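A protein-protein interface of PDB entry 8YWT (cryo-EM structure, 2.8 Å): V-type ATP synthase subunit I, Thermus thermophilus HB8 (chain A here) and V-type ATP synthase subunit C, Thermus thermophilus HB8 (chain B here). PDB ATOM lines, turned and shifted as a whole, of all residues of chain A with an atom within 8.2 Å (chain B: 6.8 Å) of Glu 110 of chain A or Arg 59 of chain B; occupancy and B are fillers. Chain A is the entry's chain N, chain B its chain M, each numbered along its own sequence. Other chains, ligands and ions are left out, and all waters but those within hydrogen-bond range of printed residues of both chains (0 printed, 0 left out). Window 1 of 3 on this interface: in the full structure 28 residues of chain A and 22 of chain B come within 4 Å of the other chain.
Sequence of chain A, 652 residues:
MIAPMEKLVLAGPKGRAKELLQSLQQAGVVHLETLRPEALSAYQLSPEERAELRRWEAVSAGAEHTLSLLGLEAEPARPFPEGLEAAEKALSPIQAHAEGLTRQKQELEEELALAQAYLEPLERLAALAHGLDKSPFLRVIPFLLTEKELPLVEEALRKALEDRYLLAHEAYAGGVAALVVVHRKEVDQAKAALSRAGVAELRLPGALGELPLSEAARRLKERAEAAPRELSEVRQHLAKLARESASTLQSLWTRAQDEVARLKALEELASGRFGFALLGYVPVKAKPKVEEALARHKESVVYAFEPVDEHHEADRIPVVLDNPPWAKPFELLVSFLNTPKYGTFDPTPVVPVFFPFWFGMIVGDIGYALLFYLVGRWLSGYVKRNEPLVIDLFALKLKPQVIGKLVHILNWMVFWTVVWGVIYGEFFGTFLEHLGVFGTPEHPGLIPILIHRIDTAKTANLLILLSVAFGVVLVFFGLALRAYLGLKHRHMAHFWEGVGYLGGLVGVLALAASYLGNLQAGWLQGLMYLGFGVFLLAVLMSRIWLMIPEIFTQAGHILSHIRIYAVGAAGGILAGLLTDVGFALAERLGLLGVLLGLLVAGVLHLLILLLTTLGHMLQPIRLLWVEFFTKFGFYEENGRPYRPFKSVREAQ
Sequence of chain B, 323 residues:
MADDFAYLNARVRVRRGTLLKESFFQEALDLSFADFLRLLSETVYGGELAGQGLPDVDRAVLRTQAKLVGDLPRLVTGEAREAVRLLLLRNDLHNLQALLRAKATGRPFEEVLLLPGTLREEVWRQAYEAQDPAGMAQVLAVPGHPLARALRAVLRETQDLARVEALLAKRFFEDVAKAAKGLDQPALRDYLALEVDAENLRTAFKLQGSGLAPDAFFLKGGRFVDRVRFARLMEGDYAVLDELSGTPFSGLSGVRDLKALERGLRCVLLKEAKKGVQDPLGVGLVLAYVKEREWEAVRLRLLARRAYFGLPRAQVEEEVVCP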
ATOM      1  N   GLU A  99      -7.357 -20.356 -14.094  1.00  0.00           N
ATOM      2  CA  GLU A  99      -7.193 -19.915 -12.708  1.00  0.00           C
ATOM      3  C   GLU A  99      -5.754 -19.483 -12.417  1.00  0.00           C
ATOM      4  O   GLU A  99      -5.563 -18.471 -11.757  1.00  0.00           O
ATOM      5  CB  GLU A  99      -7.604 -21.037 -11.744  1.00  0.00           C
ATOM      6  CG  GLU A  99      -9.123 -21.257 -11.676  1.00  0.00           C
ATOM      7  CD  GLU A  99      -9.502 -22.444 -10.773  1.00  0.00           C
ATOM      8  OE1 GLU A  99      -8.643 -22.977 -10.044  1.00  0.00           O
ATOM      9  OE2 GLU A  99     -10.685 -22.858 -10.748  1.00  0.00           O
ATOM     10  N   GLY A 100      -4.743 -20.173 -12.945  1.00  0.00           N
ATOM     11  CA  GLY A 100      -3.342 -19.781 -12.803  1.00  0.00           C
ATOM     12  C   GLY A 100      -3.021 -18.424 -13.437  1.00  0.00           C
ATOM     13  O   GLY A 100      -2.433 -17.565 -12.784  1.00  0.00           O
ATOM     14  N   THR A 102      -5.293 -15.994 -14.098  1.00  0.00           N
ATOM     15  CA  THR A 102      -6.019 -15.022 -13.269  1.00  0.00           C
ATOM     16  C   THR A 102      -5.323 -14.786 -11.934  1.00  0.00           C
ATOM     17  O   THR A 102      -5.244 -13.648 -11.488  1.00  0.00           O
ATOM     18  CB  THR A 102      -7.469 -15.464 -13.047  1.00  0.00           C
ATOM     19  OG1 THR A 102      -8.128 -15.572 -14.282  1.00  0.00           O
ATOM     20  CG2 THR A 102      -8.289 -14.488 -12.216  1.00  0.00           C
ATOM     21  N   ARG A 103      -4.747 -15.810 -11.301  1.00  0.00           N
ATOM     22  CA  ARG A 103      -3.984 -15.672 -10.055  1.00  0.00           C
ATOM     23  C   ARG A 103      -2.722 -14.842 -10.258  1.00  0.00           C
ATOM     24  O   ARG A 103      -2.470 -13.949  -9.458  1.00  0.00           O
ATOM     25  CB  ARG A 103      -3.706 -17.073  -9.493  1.00  0.00           C
ATOM     26  CG  ARG A 103      -3.033 -17.029  -8.119  1.00  0.00           C
ATOM     27  CD  ARG A 103      -3.194 -18.348  -7.358  1.00  0.00           C
ATOM     28  NE  ARG A 103      -2.459 -19.463  -7.983  1.00  0.00           N
ATOM     29  CZ  ARG A 103      -2.937 -20.623  -8.395  1.00  0.00           C
ATOM     30  NH1 ARG A 103      -2.119 -21.559  -8.761  1.00  0.00           N
ATOM     31  NH2 ARG A 103      -4.209 -20.892  -8.468  1.00  0.00           N
ATOM     32  N   GLN A 104      -1.995 -15.034 -11.364  1.00  0.00           N
ATOM     33  CA  GLN A 104      -0.888 -14.151 -11.744  1.00  0.00           C
ATOM     34  C   GLN A 104      -1.362 -12.705 -11.902  1.00  0.00           C
ATOM     35  O   GLN A 104      -0.801 -11.806 -11.284  1.00  0.00           O
ATOM     36  CB  GLN A 104      -0.222 -14.613 -13.049  1.00  0.00           C
ATOM     37  CG  GLN A 104       0.639 -15.871 -12.881  1.00  0.00           C
ATOM     38  CD  GLN A 104       1.220 -16.373 -14.201  1.00  0.00           C
ATOM     39  OE1 GLN A 104       1.133 -17.542 -14.543  1.00  0.00           O
ATOM     40  NE2 GLN A 104       1.815 -15.528 -15.007  1.00  0.00           N
ATOM     41  N   LYS A 105      -2.430 -12.476 -12.672  1.00  0.00           N
ATOM     42  CA  LYS A 105      -2.968 -11.136 -12.931  1.00  0.00           C
ATOM     43  C   LYS A 105      -3.329 -10.403 -11.639  1.00  0.00           C
ATOM     44  O   LYS A 105      -2.913  -9.267 -11.457  1.00  0.00           O
ATOM     45  CB  LYS A 105      -4.167 -11.262 -13.878  1.00  0.00           C
ATOM     46  CG  LYS A 105      -4.506  -9.921 -14.541  1.00  0.00           C
ATOM     47  CD  LYS A 105      -5.715 -10.031 -15.485  1.00  0.00           C
ATOM     48  CE  LYS A 105      -7.065 -10.164 -14.764  1.00  0.00           C
ATOM     49  NZ  LYS A 105      -7.567  -8.862 -14.248  1.00  0.00           N
ATOM     50  N   GLN A 106      -4.020 -11.061 -10.708  1.00  0.00           N
ATOM     51  CA  GLN A 106      -4.396 -10.474  -9.420  1.00  0.00           C
ATOM     52  C   GLN A 106      -3.173 -10.048  -8.597  1.00  0.00           C
ATOM     53  O   GLN A 106      -3.187  -8.997  -7.969  1.00  0.00           O
ATOM     54  CB  GLN A 106      -5.267 -11.460  -8.622  1.00  0.00           C
ATOM     55  CG  GLN A 106      -6.677 -11.616  -9.224  1.00  0.00           C
ATOM     56  CD  GLN A 106      -7.595 -12.649  -8.558  1.00  0.00           C
ATOM     57  OE1 GLN A 106      -8.689 -12.916  -9.021  1.00  0.00           O
ATOM     58  NE2 GLN A 106      -7.219 -13.291  -7.476  1.00  0.00           N
ATOM     59  N   GLU A 107      -2.086 -10.816  -8.594  1.00  0.00           N
ATOM     60  CA  GLU A 107      -0.898 -10.469  -7.803  1.00  0.00           C
ATOM     61  C   GLU A 107      -0.032  -9.386  -8.450  1.00  0.00           C
ATOM     62  O   GLU A 107       0.538  -8.557  -7.743  1.00  0.00           O
ATOM     63  CB  GLU A 107      -0.078 -11.724  -7.518  1.00  0.00           C
ATOM     64  CG  GLU A 107      -0.874 -12.603  -6.555  1.00  0.00           C
ATOM     65  CD  GLU A 107      -0.223 -13.943  -6.229  1.00  0.00           C
ATOM     66  OE1 GLU A 107       1.013 -14.092  -6.356  1.00  0.00           O
ATOM     67  OE2 GLU A 107      -0.984 -14.837  -5.799  1.00  0.00           O
ATOM     68  N   LEU A 108       0.028  -9.336  -9.780  1.00  0.00           N
ATOM     69  CA  LEU A 108       0.641  -8.212 -10.494  1.00  0.00           C
ATOM     70  C   LEU A 108      -0.111  -6.902 -10.207  1.00  0.00           C
ATOM     71  O   LEU A 108       0.526  -5.882  -9.957  1.00  0.00           O
ATOM     72  CB  LEU A 108       0.671  -8.512 -12.000  1.00  0.00           C
ATOM     73  CG  LEU A 108       1.982  -9.128 -12.513  1.00  0.00           C
ATOM     74  CD1 LEU A 108       2.402 -10.397 -11.778  1.00  0.00           C
ATOM     75  CD2 LEU A 108       1.826  -9.479 -13.989  1.00  0.00           C
ATOM     76  N   GLU A 109      -1.448  -6.930 -10.192  1.00  0.00           N
ATOM     77  CA  GLU A 109      -2.272  -5.787  -9.785  1.00  0.00           C
ATOM     78  C   GLU A 109      -1.955  -5.335  -8.354  1.00  0.00           C
ATOM     79  O   GLU A 109      -1.747  -4.148  -8.116  1.00  0.00           O
ATOM     80  CB  GLU A 109      -3.767  -6.139  -9.857  1.00  0.00           C
ATOM     81  CG  GLU A 109      -4.337  -6.305 -11.271  1.00  0.00           C
ATOM     82  CD  GLU A 109      -5.747  -6.934 -11.267  1.00  0.00           C
ATOM     83  OE1 GLU A 109      -6.421  -6.948 -10.211  1.00  0.00           O
ATOM     84  OE2 GLU A 109      -6.213  -7.381 -12.340  1.00  0.00           O
ATOM     85  N   GLU A 110      -1.907  -6.265  -7.398  1.00  0.00           N
ATOM     86  CA  GLU A 110      -1.653  -5.964  -5.984  1.00  0.00           C
ATOM     87  C   GLU A 110      -0.234  -5.402  -5.739  1.00  0.00           C
ATOM     88  O   GLU A 110      -0.068  -4.454  -4.976  1.00  0.00           O
ATOM     89  CB  GLU A 110      -1.912  -7.230  -5.146  1.00  0.00           C
ATOM     90  CG  GLU A 110      -3.414  -7.590  -5.082  1.00  0.00           C
ATOM     91  CD  GLU A 110      -3.712  -9.055  -4.698  1.00  0.00           C
ATOM     92  OE1 GLU A 110      -2.877  -9.707  -4.035  1.00  0.00           O
ATOM     93  OE2 GLU A 110      -4.811  -9.561  -5.034  1.00  0.00           O
ATOM     94  N   GLU A 111       0.795  -5.925  -6.417  1.00  0.00           N
ATOM     95  CA  GLU A 111       2.156  -5.395  -6.348  1.00  0.00           C
ATOM     96  C   GLU A 111       2.249  -3.962  -6.900  1.00  0.00           C
ATOM     97  O   GLU A 111       2.810  -3.082  -6.247  1.00  0.00           O
ATOM     98  CB  GLU A 111       3.086  -6.348  -7.106  1.00  0.00           C
ATOM     99  CG  GLU A 111       4.552  -5.907  -7.080  1.00  0.00           C
ATOM    100  CD  GLU A 111       5.410  -6.753  -8.021  1.00  0.00           C
ATOM    101  OE1 GLU A 111       5.407  -7.997  -7.910  1.00  0.00           O
ATOM    102  OE2 GLU A 111       6.101  -6.166  -8.879  1.00  0.00           O
ATOM    103  N   LEU A 112       1.678  -3.708  -8.082  1.00  0.00           N
ATOM    104  CA  LEU A 112       1.683  -2.388  -8.707  1.00  0.00           C
ATOM    105  C   LEU A 112       0.947  -1.348  -7.852  1.00  0.00           C
ATOM    106  O   LEU A 112       1.456  -0.248  -7.643  1.00  0.00           O
ATOM    107  CB  LEU A 112       1.077  -2.528 -10.112  1.00  0.00           C
ATOM    108  CG  LEU A 112       0.879  -1.213 -10.879  1.00  0.00           C
ATOM    109  CD1 LEU A 112       2.180  -0.436 -11.069  1.00  0.00           C
ATOM    110  CD2 LEU A 112       0.311  -1.521 -12.259  1.00  0.00           C
ATOM    111  N   ALA A 113      -0.217  -1.705  -7.307  1.00  0.00           N
ATOM    112  CA  ALA A 113      -1.002  -0.837  -6.436  1.00  0.00           C
ATOM    113  C   ALA A 113      -0.227  -0.388  -5.186  1.00  0.00           C
ATOM    114  O   ALA A 113      -0.223   0.797  -4.859  1.00  0.00           O
ATOM    115  CB  ALA A 113      -2.280  -1.580  -6.049  1.00  0.00           C
ATOM    116  N   LEU A 114       0.455  -1.310  -4.499  1.00  0.00           N
ATOM    117  CA  LEU A 114       1.215  -0.972  -3.298  1.00  0.00           C
ATOM    118  C   LEU A 114       2.467  -0.151  -3.624  1.00  0.00           C
ATOM    119  O   LEU A 114       2.777   0.806  -2.916  1.00  0.00           O
ATOM    120  CB  LEU A 114       1.544  -2.269  -2.544  1.00  0.00           C
ATOM    121  CG  LEU A 114       2.067  -2.049  -1.113  1.00  0.00           C
ATOM    122  CD1 LEU A 114       1.016  -1.417  -0.196  1.00  0.00           C
ATOM    123  CD2 LEU A 114       2.446  -3.393  -0.505  1.00  0.00           C
ATOM    124  N   ALA A 115       3.163  -0.476  -4.717  1.00  0.00           N
ATOM    125  CA  ALA A 115       4.348   0.258  -5.147  1.00  0.00           C
ATOM    126  C   ALA A 115       4.020   1.714  -5.490  1.00  0.00           C
ATOM    127  O   ALA A 115       4.657   2.619  -4.959  1.00  0.00           O
ATOM    128  CB  ALA A 115       4.992  -0.468  -6.332  1.00  0.00           C
ATOM    129  N   GLN A 116       2.998   1.972  -6.311  1.00  0.00           N
ATOM    130  CA  GLN A 116       2.660   3.344  -6.710  1.00  0.00           C
ATOM    131  C   GLN A 116       2.143   4.227  -5.555  1.00  0.00           C
ATOM    132  O   GLN A 116       2.234   5.449  -5.642  1.00  0.00           O
ATOM    133  CB  GLN A 116       1.718   3.329  -7.927  1.00  0.00           C
ATOM    134  CG  GLN A 116       0.259   2.945  -7.629  1.00  0.00           C
ATOM    135  CD  GLN A 116      -0.632   2.899  -8.872  1.00  0.00           C
ATOM    136  OE1 GLN A 116      -0.228   3.156  -9.997  1.00  0.00           O
ATOM    137  NE2 GLN A 116      -1.898   2.590  -8.716  1.00  0.00           N
ATOM    138  N   LEU A 231       1.509  -7.042 -17.024  1.00  0.00           N
ATOM    139  CA  LEU A 231       0.049  -7.120 -17.157  1.00  0.00           C
ATOM    140  C   LEU A 231      -0.347  -7.336 -18.622  1.00  0.00           C
ATOM    141  O   LEU A 231      -1.176  -8.194 -18.914  1.00  0.00           O
ATOM    142  CB  LEU A 231      -0.668  -5.870 -16.594  1.00  0.00           C
ATOM    143  CG  LEU A 231      -0.971  -5.791 -15.084  1.00  0.00           C
ATOM    144  CD1 LEU A 231      -1.592  -7.075 -14.537  1.00  0.00           C
ATOM    145  CD2 LEU A 231       0.239  -5.422 -14.241  1.00  0.00           C
ATOM    146  N   GLU B  48     -13.779 -13.554  -9.084  1.00  0.00           N
ATOM    147  CA  GLU B  48     -12.523 -13.435  -8.322  1.00  0.00           C
ATOM    148  C   GLU B  48     -12.014 -14.779  -7.763  1.00  0.00           C
ATOM    149  O   GLU B  48     -11.057 -14.802  -6.993  1.00  0.00           O
ATOM    150  CB  GLU B  48     -12.704 -12.431  -7.174  1.00  0.00           C
ATOM    151  CG  GLU B  48     -13.157 -11.027  -7.583  1.00  0.00           C
ATOM    152  CD  GLU B  48     -12.107 -10.215  -8.353  1.00  0.00           C
ATOM    153  OE1 GLU B  48     -10.919 -10.205  -7.971  1.00  0.00           O
ATOM    154  OE2 GLU B  48     -12.502  -9.525  -9.319  1.00  0.00           O
ATOM    155  N   LEU B  49     -12.635 -15.912  -8.097  1.00  0.00           N
ATOM    156  CA  LEU B  49     -12.094 -17.231  -7.757  1.00  0.00           C
ATOM    157  C   LEU B  49     -10.977 -17.607  -8.733  1.00  0.00           C
ATOM    158  O   LEU B  49     -11.209 -17.757  -9.921  1.00  0.00           O
ATOM    159  CB  LEU B  49     -13.196 -18.304  -7.745  1.00  0.00           C
ATOM    160  CG  LEU B  49     -13.885 -18.519  -6.392  1.00  0.00           C
ATOM    161  CD1 LEU B  49     -15.049 -19.486  -6.583  1.00  0.00           C
ATOM    162  CD2 LEU B  49     -12.946 -19.132  -5.357  1.00  0.00           C
ATOM    163  N   ALA B  50      -9.767 -17.791  -8.219  1.00  0.00           N
ATOM    164  CA  ALA B  50      -8.561 -18.071  -8.993  1.00  0.00           C
ATOM    165  C   ALA B  50      -7.776 -19.240  -8.382  1.00  0.00           C
ATOM    166  O   ALA B  50      -6.547 -19.250  -8.358  1.00  0.00           O
ATOM    167  CB  ALA B  50      -7.740 -16.787  -9.107  1.00  0.00           C
ATOM    168  N   LEU B  54      -8.908 -22.711   0.710  1.00  0.00           N
ATOM    169  CA  LEU B  54      -9.459 -21.717   1.629  1.00  0.00           C
ATOM    170  C   LEU B  54      -8.867 -20.296   1.453  1.00  0.00           C
ATOM    171  O   LEU B  54      -9.640 -19.338   1.475  1.00  0.00           O
ATOM    172  CB  LEU B  54      -9.356 -22.280   3.055  1.00  0.00           C
ATOM    173  CG  LEU B  54     -10.104 -21.469   4.119  1.00  0.00           C
ATOM    174  CD1 LEU B  54     -11.611 -21.454   3.877  1.00  0.00           C
ATOM    175  CD2 LEU B  54      -9.847 -22.095   5.483  1.00  0.00           C
ATOM    176  N   PRO B  55      -7.565 -20.106   1.160  1.00  0.00           N
ATOM    177  CA  PRO B  55      -7.028 -18.791   0.818  1.00  0.00           C
ATOM    178  C   PRO B  55      -7.652 -18.162  -0.434  1.00  0.00           C
ATOM    179  O   PRO B  55      -7.771 -16.945  -0.526  1.00  0.00           O
ATOM    180  CB  PRO B  55      -5.527 -19.008   0.615  1.00  0.00           C
ATOM    181  CG  PRO B  55      -5.221 -20.221   1.478  1.00  0.00           C
ATOM    182  CD  PRO B  55      -6.477 -21.059   1.306  1.00  0.00           C
ATOM    183  N   ASP B  56      -8.078 -18.972  -1.405  1.00  0.00           N
ATOM    184  CA  ASP B  56      -8.694 -18.492  -2.642  1.00  0.00           C
ATOM    185  C   ASP B  56     -10.142 -18.069  -2.448  1.00  0.00           C
ATOM    186  O   ASP B  56     -10.557 -17.073  -3.038  1.00  0.00           O
ATOM    187  CB  ASP B  56      -8.618 -19.560  -3.724  1.00  0.00           C
ATOM    188  CG  ASP B  56      -7.201 -20.096  -3.861  1.00  0.00           C
ATOM    189  OD1 ASP B  56      -6.336 -19.350  -4.364  1.00  0.00           O
ATOM    190  OD2 ASP B  56      -6.978 -21.258  -3.469  1.00  0.00           O
ATOM    191  N   VAL B  57     -10.903 -18.766  -1.607  1.00  0.00           N
ATOM    192  CA  VAL B  57     -12.227 -18.289  -1.196  1.00  0.00           C
ATOM    193  C   VAL B  57     -12.101 -16.964  -0.467  1.00  0.00           C
ATOM    194  O   VAL B  57     -12.776 -16.008  -0.832  1.00  0.00           O
ATOM    195  CB  VAL B  57     -12.956 -19.320  -0.326  1.00  0.00           C
ATOM    196  CG1 VAL B  57     -14.217 -18.738   0.312  1.00  0.00           C
ATOM    197  CG2 VAL B  57     -13.372 -20.511  -1.183  1.00  0.00           C
ATOM    198  N   ASP B  58     -11.200 -16.862   0.508  1.00  0.00           N
ATOM    199  CA  ASP B  58     -11.020 -15.635   1.279  1.00  0.00           C
ATOM    200  C   ASP B  58     -10.633 -14.454   0.388  1.00  0.00           C
ATOM    201  O   ASP B  58     -11.268 -13.403   0.463  1.00  0.00           O
ATOM    202  CB  ASP B  58     -10.005 -15.878   2.402  1.00  0.00           C
ATOM    203  CG  ASP B  58     -10.530 -16.812   3.502  1.00  0.00           C
ATOM    204  OD1 ASP B  58     -11.752 -17.049   3.566  1.00  0.00           O
ATOM    205  OD2 ASP B  58      -9.747 -17.225   4.386  1.00  0.00           O
ATOM    206  N   ARG B  59      -9.679 -14.636  -0.532  1.00  0.00           N
ATOM    207  CA  ARG B  59      -9.319 -13.607  -1.514  1.00  0.00           C
ATOM    208  C   ARG B  59     -10.463 -13.268  -2.466  1.00  0.00           C
ATOM    209  O   ARG B  59     -10.612 -12.103  -2.816  1.00  0.00           O
ATOM    210  CB  ARG B  59      -8.031 -14.003  -2.251  1.00  0.00           C
ATOM    211  CG  ARG B  59      -7.580 -12.872  -3.191  1.00  0.00           C
ATOM    212  CD  ARG B  59      -6.070 -12.645  -3.291  1.00  0.00           C
ATOM    213  NE  ARG B  59      -5.381 -13.680  -4.074  1.00  0.00           N
ATOM    214  CZ  ARG B  59      -4.347 -13.509  -4.880  1.00  0.00           C
ATOM    215  NH1 ARG B  59      -3.726 -14.551  -5.338  1.00  0.00           N
ATOM    216  NH2 ARG B  59      -3.928 -12.339  -5.261  1.00  0.00           N
ATOM    217  N   ALA B  60     -11.311 -14.217  -2.850  1.00  0.00           N
ATOM    218  CA  ALA B  60     -12.472 -13.932  -3.685  1.00  0.00           C
ATOM    219  C   ALA B  60     -13.507 -13.050  -2.976  1.00  0.00           C
ATOM    220  O   ALA B  60     -14.040 -12.131  -3.593  1.00  0.00           O
ATOM    221  CB  ALA B  60     -13.090 -15.250  -4.152  1.00  0.00           C
ATOM    222  N   VAL B  61     -13.768 -13.271  -1.685  1.00  0.00           N
ATOM    223  CA  VAL B  61     -14.695 -12.446  -0.892  1.00  0.00           C
ATOM    224  C   VAL B  61     -14.135 -11.049  -0.675  1.00  0.00           C
ATOM    225  O   VAL B  61     -14.826 -10.067  -0.943  1.00  0.00           O
ATOM    226  CB  VAL B  61     -15.055 -13.105   0.449  1.00  0.00           C
ATOM    227  CG1 VAL B  61     -15.962 -12.205   1.289  1.00  0.00           C
ATOM    228  CG2 VAL B  61     -15.802 -14.423   0.235  1.00  0.00           C
ATOM    229  N   LEU B  62     -12.862 -10.939  -0.290  1.00  0.00           N
ATOM    230  CA  LEU B  62     -12.177  -9.656  -0.145  1.00  0.00           C
ATOM    231  C   LEU B  62     -12.236  -8.844  -1.440  1.00  0.00           C
ATOM    232  O   LEU B  62     -12.714  -7.709  -1.444  1.00  0.00           O
ATOM    233  CB  LEU B  62     -10.718  -9.896   0.279  1.00  0.00           C
ATOM    234  CG  LEU B  62     -10.554 -10.214   1.773  1.00  0.00           C
ATOM    235  CD1 LEU B  62      -9.275 -11.006   2.022  1.00  0.00           C
ATOM    236  CD2 LEU B  62     -10.471  -8.928   2.592  1.00  0.00           C
ATOM    237  N   ARG B  63     -11.771  -9.410  -2.556  1.00  0.00           N
ATOM    238  CA  ARG B  63     -11.635  -8.674  -3.817  1.00  0.00           C
ATOM    239  C   ARG B  63     -12.959  -8.333  -4.475  1.00  0.00           C
ATOM    240  O   ARG B  63     -13.072  -7.276  -5.081  1.00  0.00           O
ATOM    241  CB  ARG B  63     -10.743  -9.448  -4.782  1.00  0.00           C
ATOM    242  CG  ARG B  63      -9.271  -9.431  -4.340  1.00  0.00           C
ATOM    243  CD  ARG B  63      -8.370 -10.135  -5.352  1.00  0.00           C
ATOM    244  NE  ARG B  63      -8.509  -9.537  -6.686  1.00  0.00           N
ATOM    245  CZ  ARG B  63      -7.742  -8.643  -7.273  1.00  0.00           C
ATOM    246  NH1 ARG B  63      -8.128  -8.152  -8.406  1.00  0.00           N
ATOM    247  NH2 ARG B  63      -6.599  -8.242  -6.798  1.00  0.00           N
ATOM    248  N   THR B  64     -13.992  -9.148  -4.303  1.00  0.00           N
ATOM    249  CA  THR B  64     -15.341  -8.814  -4.785  1.00  0.00           C
ATOM    250  C   THR B  64     -15.892  -7.591  -4.061  1.00  0.00           C
ATOM    251  O   THR B  64     -16.390  -6.670  -4.698  1.00  0.00           O
ATOM    252  CB  THR B  64     -16.294  -9.998  -4.642  1.00  0.00           C
ATOM    253  OG1 THR B  64     -15.785 -11.092  -5.353  1.00  0.00           O
ATOM    254  CG2 THR B  64     -17.683  -9.713  -5.200  1.00  0.00           C
ATOM    255  N   ARG B 120      -7.771  -1.371   0.793  1.00  0.00           N
ATOM    256  CA  ARG B 120      -7.624  -2.703   0.165  1.00  0.00           C
ATOM    257  C   ARG B 120      -6.850  -3.684   1.052  1.00  0.00           C
ATOM    258  O   ARG B 120      -6.072  -3.264   1.906  1.00  0.00           O
ATOM    259  CB  ARG B 120      -6.922  -2.558  -1.194  1.00  0.00           C
ATOM    260  CG  ARG B 120      -7.861  -2.060  -2.293  1.00  0.00           C
ATOM    261  CD  ARG B 120      -7.131  -2.021  -3.642  1.00  0.00           C
ATOM    262  NE  ARG B 120      -8.070  -1.926  -4.778  1.00  0.00           N
ATOM    263  CZ  ARG B 120      -8.703  -2.919  -5.376  1.00  0.00           C
ATOM    264  NH1 ARG B 120      -8.548  -4.166  -5.030  1.00  0.00           N
ATOM    265  NH2 ARG B 120      -9.531  -2.662  -6.341  1.00  0.00           N
ATOM    266  N   GLU B 121      -7.010  -4.990   0.820  1.00  0.00           N
ATOM    267  CA  GLU B 121      -6.374  -6.043   1.630  1.00  0.00           C
ATOM    268  C   GLU B 121      -4.857  -5.886   1.740  1.00  0.00           C
ATOM    269  O   GLU B 121      -4.326  -5.976   2.841  1.00  0.00           O
ATOM    270  CB  GLU B 121      -6.698  -7.442   1.075  1.00  0.00           C
ATOM    271  CG  GLU B 121      -6.204  -8.600   1.979  1.00  0.00           C
ATOM    272  CD  GLU B 121      -5.577  -9.794   1.222  1.00  0.00           C
ATOM    273  OE1 GLU B 121      -5.989 -10.095   0.080  1.00  0.00           O
ATOM    274  OE2 GLU B 121      -4.672 -10.453   1.785  1.00  0.00           O
ATOM    275  N   GLU B 122      -4.139  -5.617   0.649  1.00  0.00           N
ATOM    276  CA  GLU B 122      -2.677  -5.539   0.702  1.00  0.00           C
ATOM    277  C   GLU B 122      -2.160  -4.412   1.598  1.00  0.00           C
ATOM    278  O   GLU B 122      -1.050  -4.518   2.103  1.00  0.00           O
ATOM    279  CB  GLU B 122      -2.048  -5.465  -0.700  1.00  0.00           C
ATOM    280  CG  GLU B 122      -2.243  -4.163  -1.495  1.00  0.00           C
ATOM    281  CD  GLU B 122      -3.614  -4.025  -2.174  1.00  0.00           C
ATOM    282  OE1 GLU B 122      -4.402  -4.993  -2.171  1.00  0.00           O
ATOM    283  OE2 GLU B 122      -3.889  -2.933  -2.714  1.00  0.00           O
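Of the printed residues of chain B, Thr 102 of chain A touches Ala 50. Of the printed residues of chain B, Gln 106 of chain A touches Glu 48, Ala 50, Arg 59 and Arg 63. Of chain B, only Arg 59 and Arg 63 come within 4 Å of Glu 110 of chain A. Of the printed residues of chain B, Ala 113 of chain A touches Glu 122. Arg 59 of chain B touches four residues of chain A. No residue of chain A comes within 4 Å of Ala 60 of chain B. Of the printed residues of chain A, Arg 63 of chain B touches Gln 106 (3.7 Å), Glu 109 (2.8 Å) and Glu 110 (2.8 Å). Of the printed residues of chain A, Glu 122 of chain B touches Ala 113. The nearest residue of chain B that does not touch Glu 110 of chain A is Glu 122 of chain B (4.02 Å). The nearest printed residue of chain B that does not touch Glu 99 of chain A is Leu 49 of chain B (4.4 Å).
The side-chain amino group (NZ) of Lys 105 of chain A lies within salt-bridge range of the side-chain carboxylate (OE2) of Glu 109 of chain A (2.8 Å). OE1 of Glu 48 of chain B lies within salt-bridge range of NE of Arg 63 of chain B, at 2.8 Å.
Among the printed residues, merely in contact across the chains: Glu 99 of chain A with Ala 50 of chain B, Thr 102 of chain A with Ala 50 of chain B, Arg 103 of chain A with Arg 59 of chain B, Gln 106 of chain A with Glu 48 of chain B, Gln 106 of chain A with Ala 50 of chain B, Gln 106 of chain A with Arg 59 of chain B, Gln 106 of chain A with Arg 63 of chain B and Ala 113 of chain A with Glu 122 of chain B.
NH2 of Arg 103 of chain A sits at hydrogen-bond distance from O of Ala 50 of chain B, 2.9 Å away. The guanidinium group (NH1) of Arg 59 of chain B is in salt-bridge range of the side-chain carboxylate (OE2) of Glu 107 of chain A (2.8 Å). The guanidinium group of Arg 63 of chain B is in salt-bridge range of the side-chain carboxylate of Glu 109 of chain A, 2.8 Å away. OE2 of Glu 110 of chain A lies within salt-bridge range of NH2 of Arg 59 of chain B (2.9 Å). The side-chain carboxylate of Glu 110 of chain A lies within salt-bridge range of the guanidinium group of Arg 63 of chain B (2.8 Å).
Hydrophobic or aromatic side chains of chain A within 4 Å of the printed part of chain B: Ala 113. Hydrophobic or aromatic side chains of chain B that line the printed part of chain A: Ala 50. Among the printed residues, 13 pairs touch across the chains. Among the printed residues, Asp or Glu carboxylates within 4 Å of a Lys or Arg side-chain nitrogen of the other chain: Glu 107 of chain A with Arg 59 of chain B, Glu 109 of chain A with Arg 63 of chain B, Glu 110 of chain A with Arg 59 of chain B and Glu 110 of chain A with Arg 63 of chain B.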
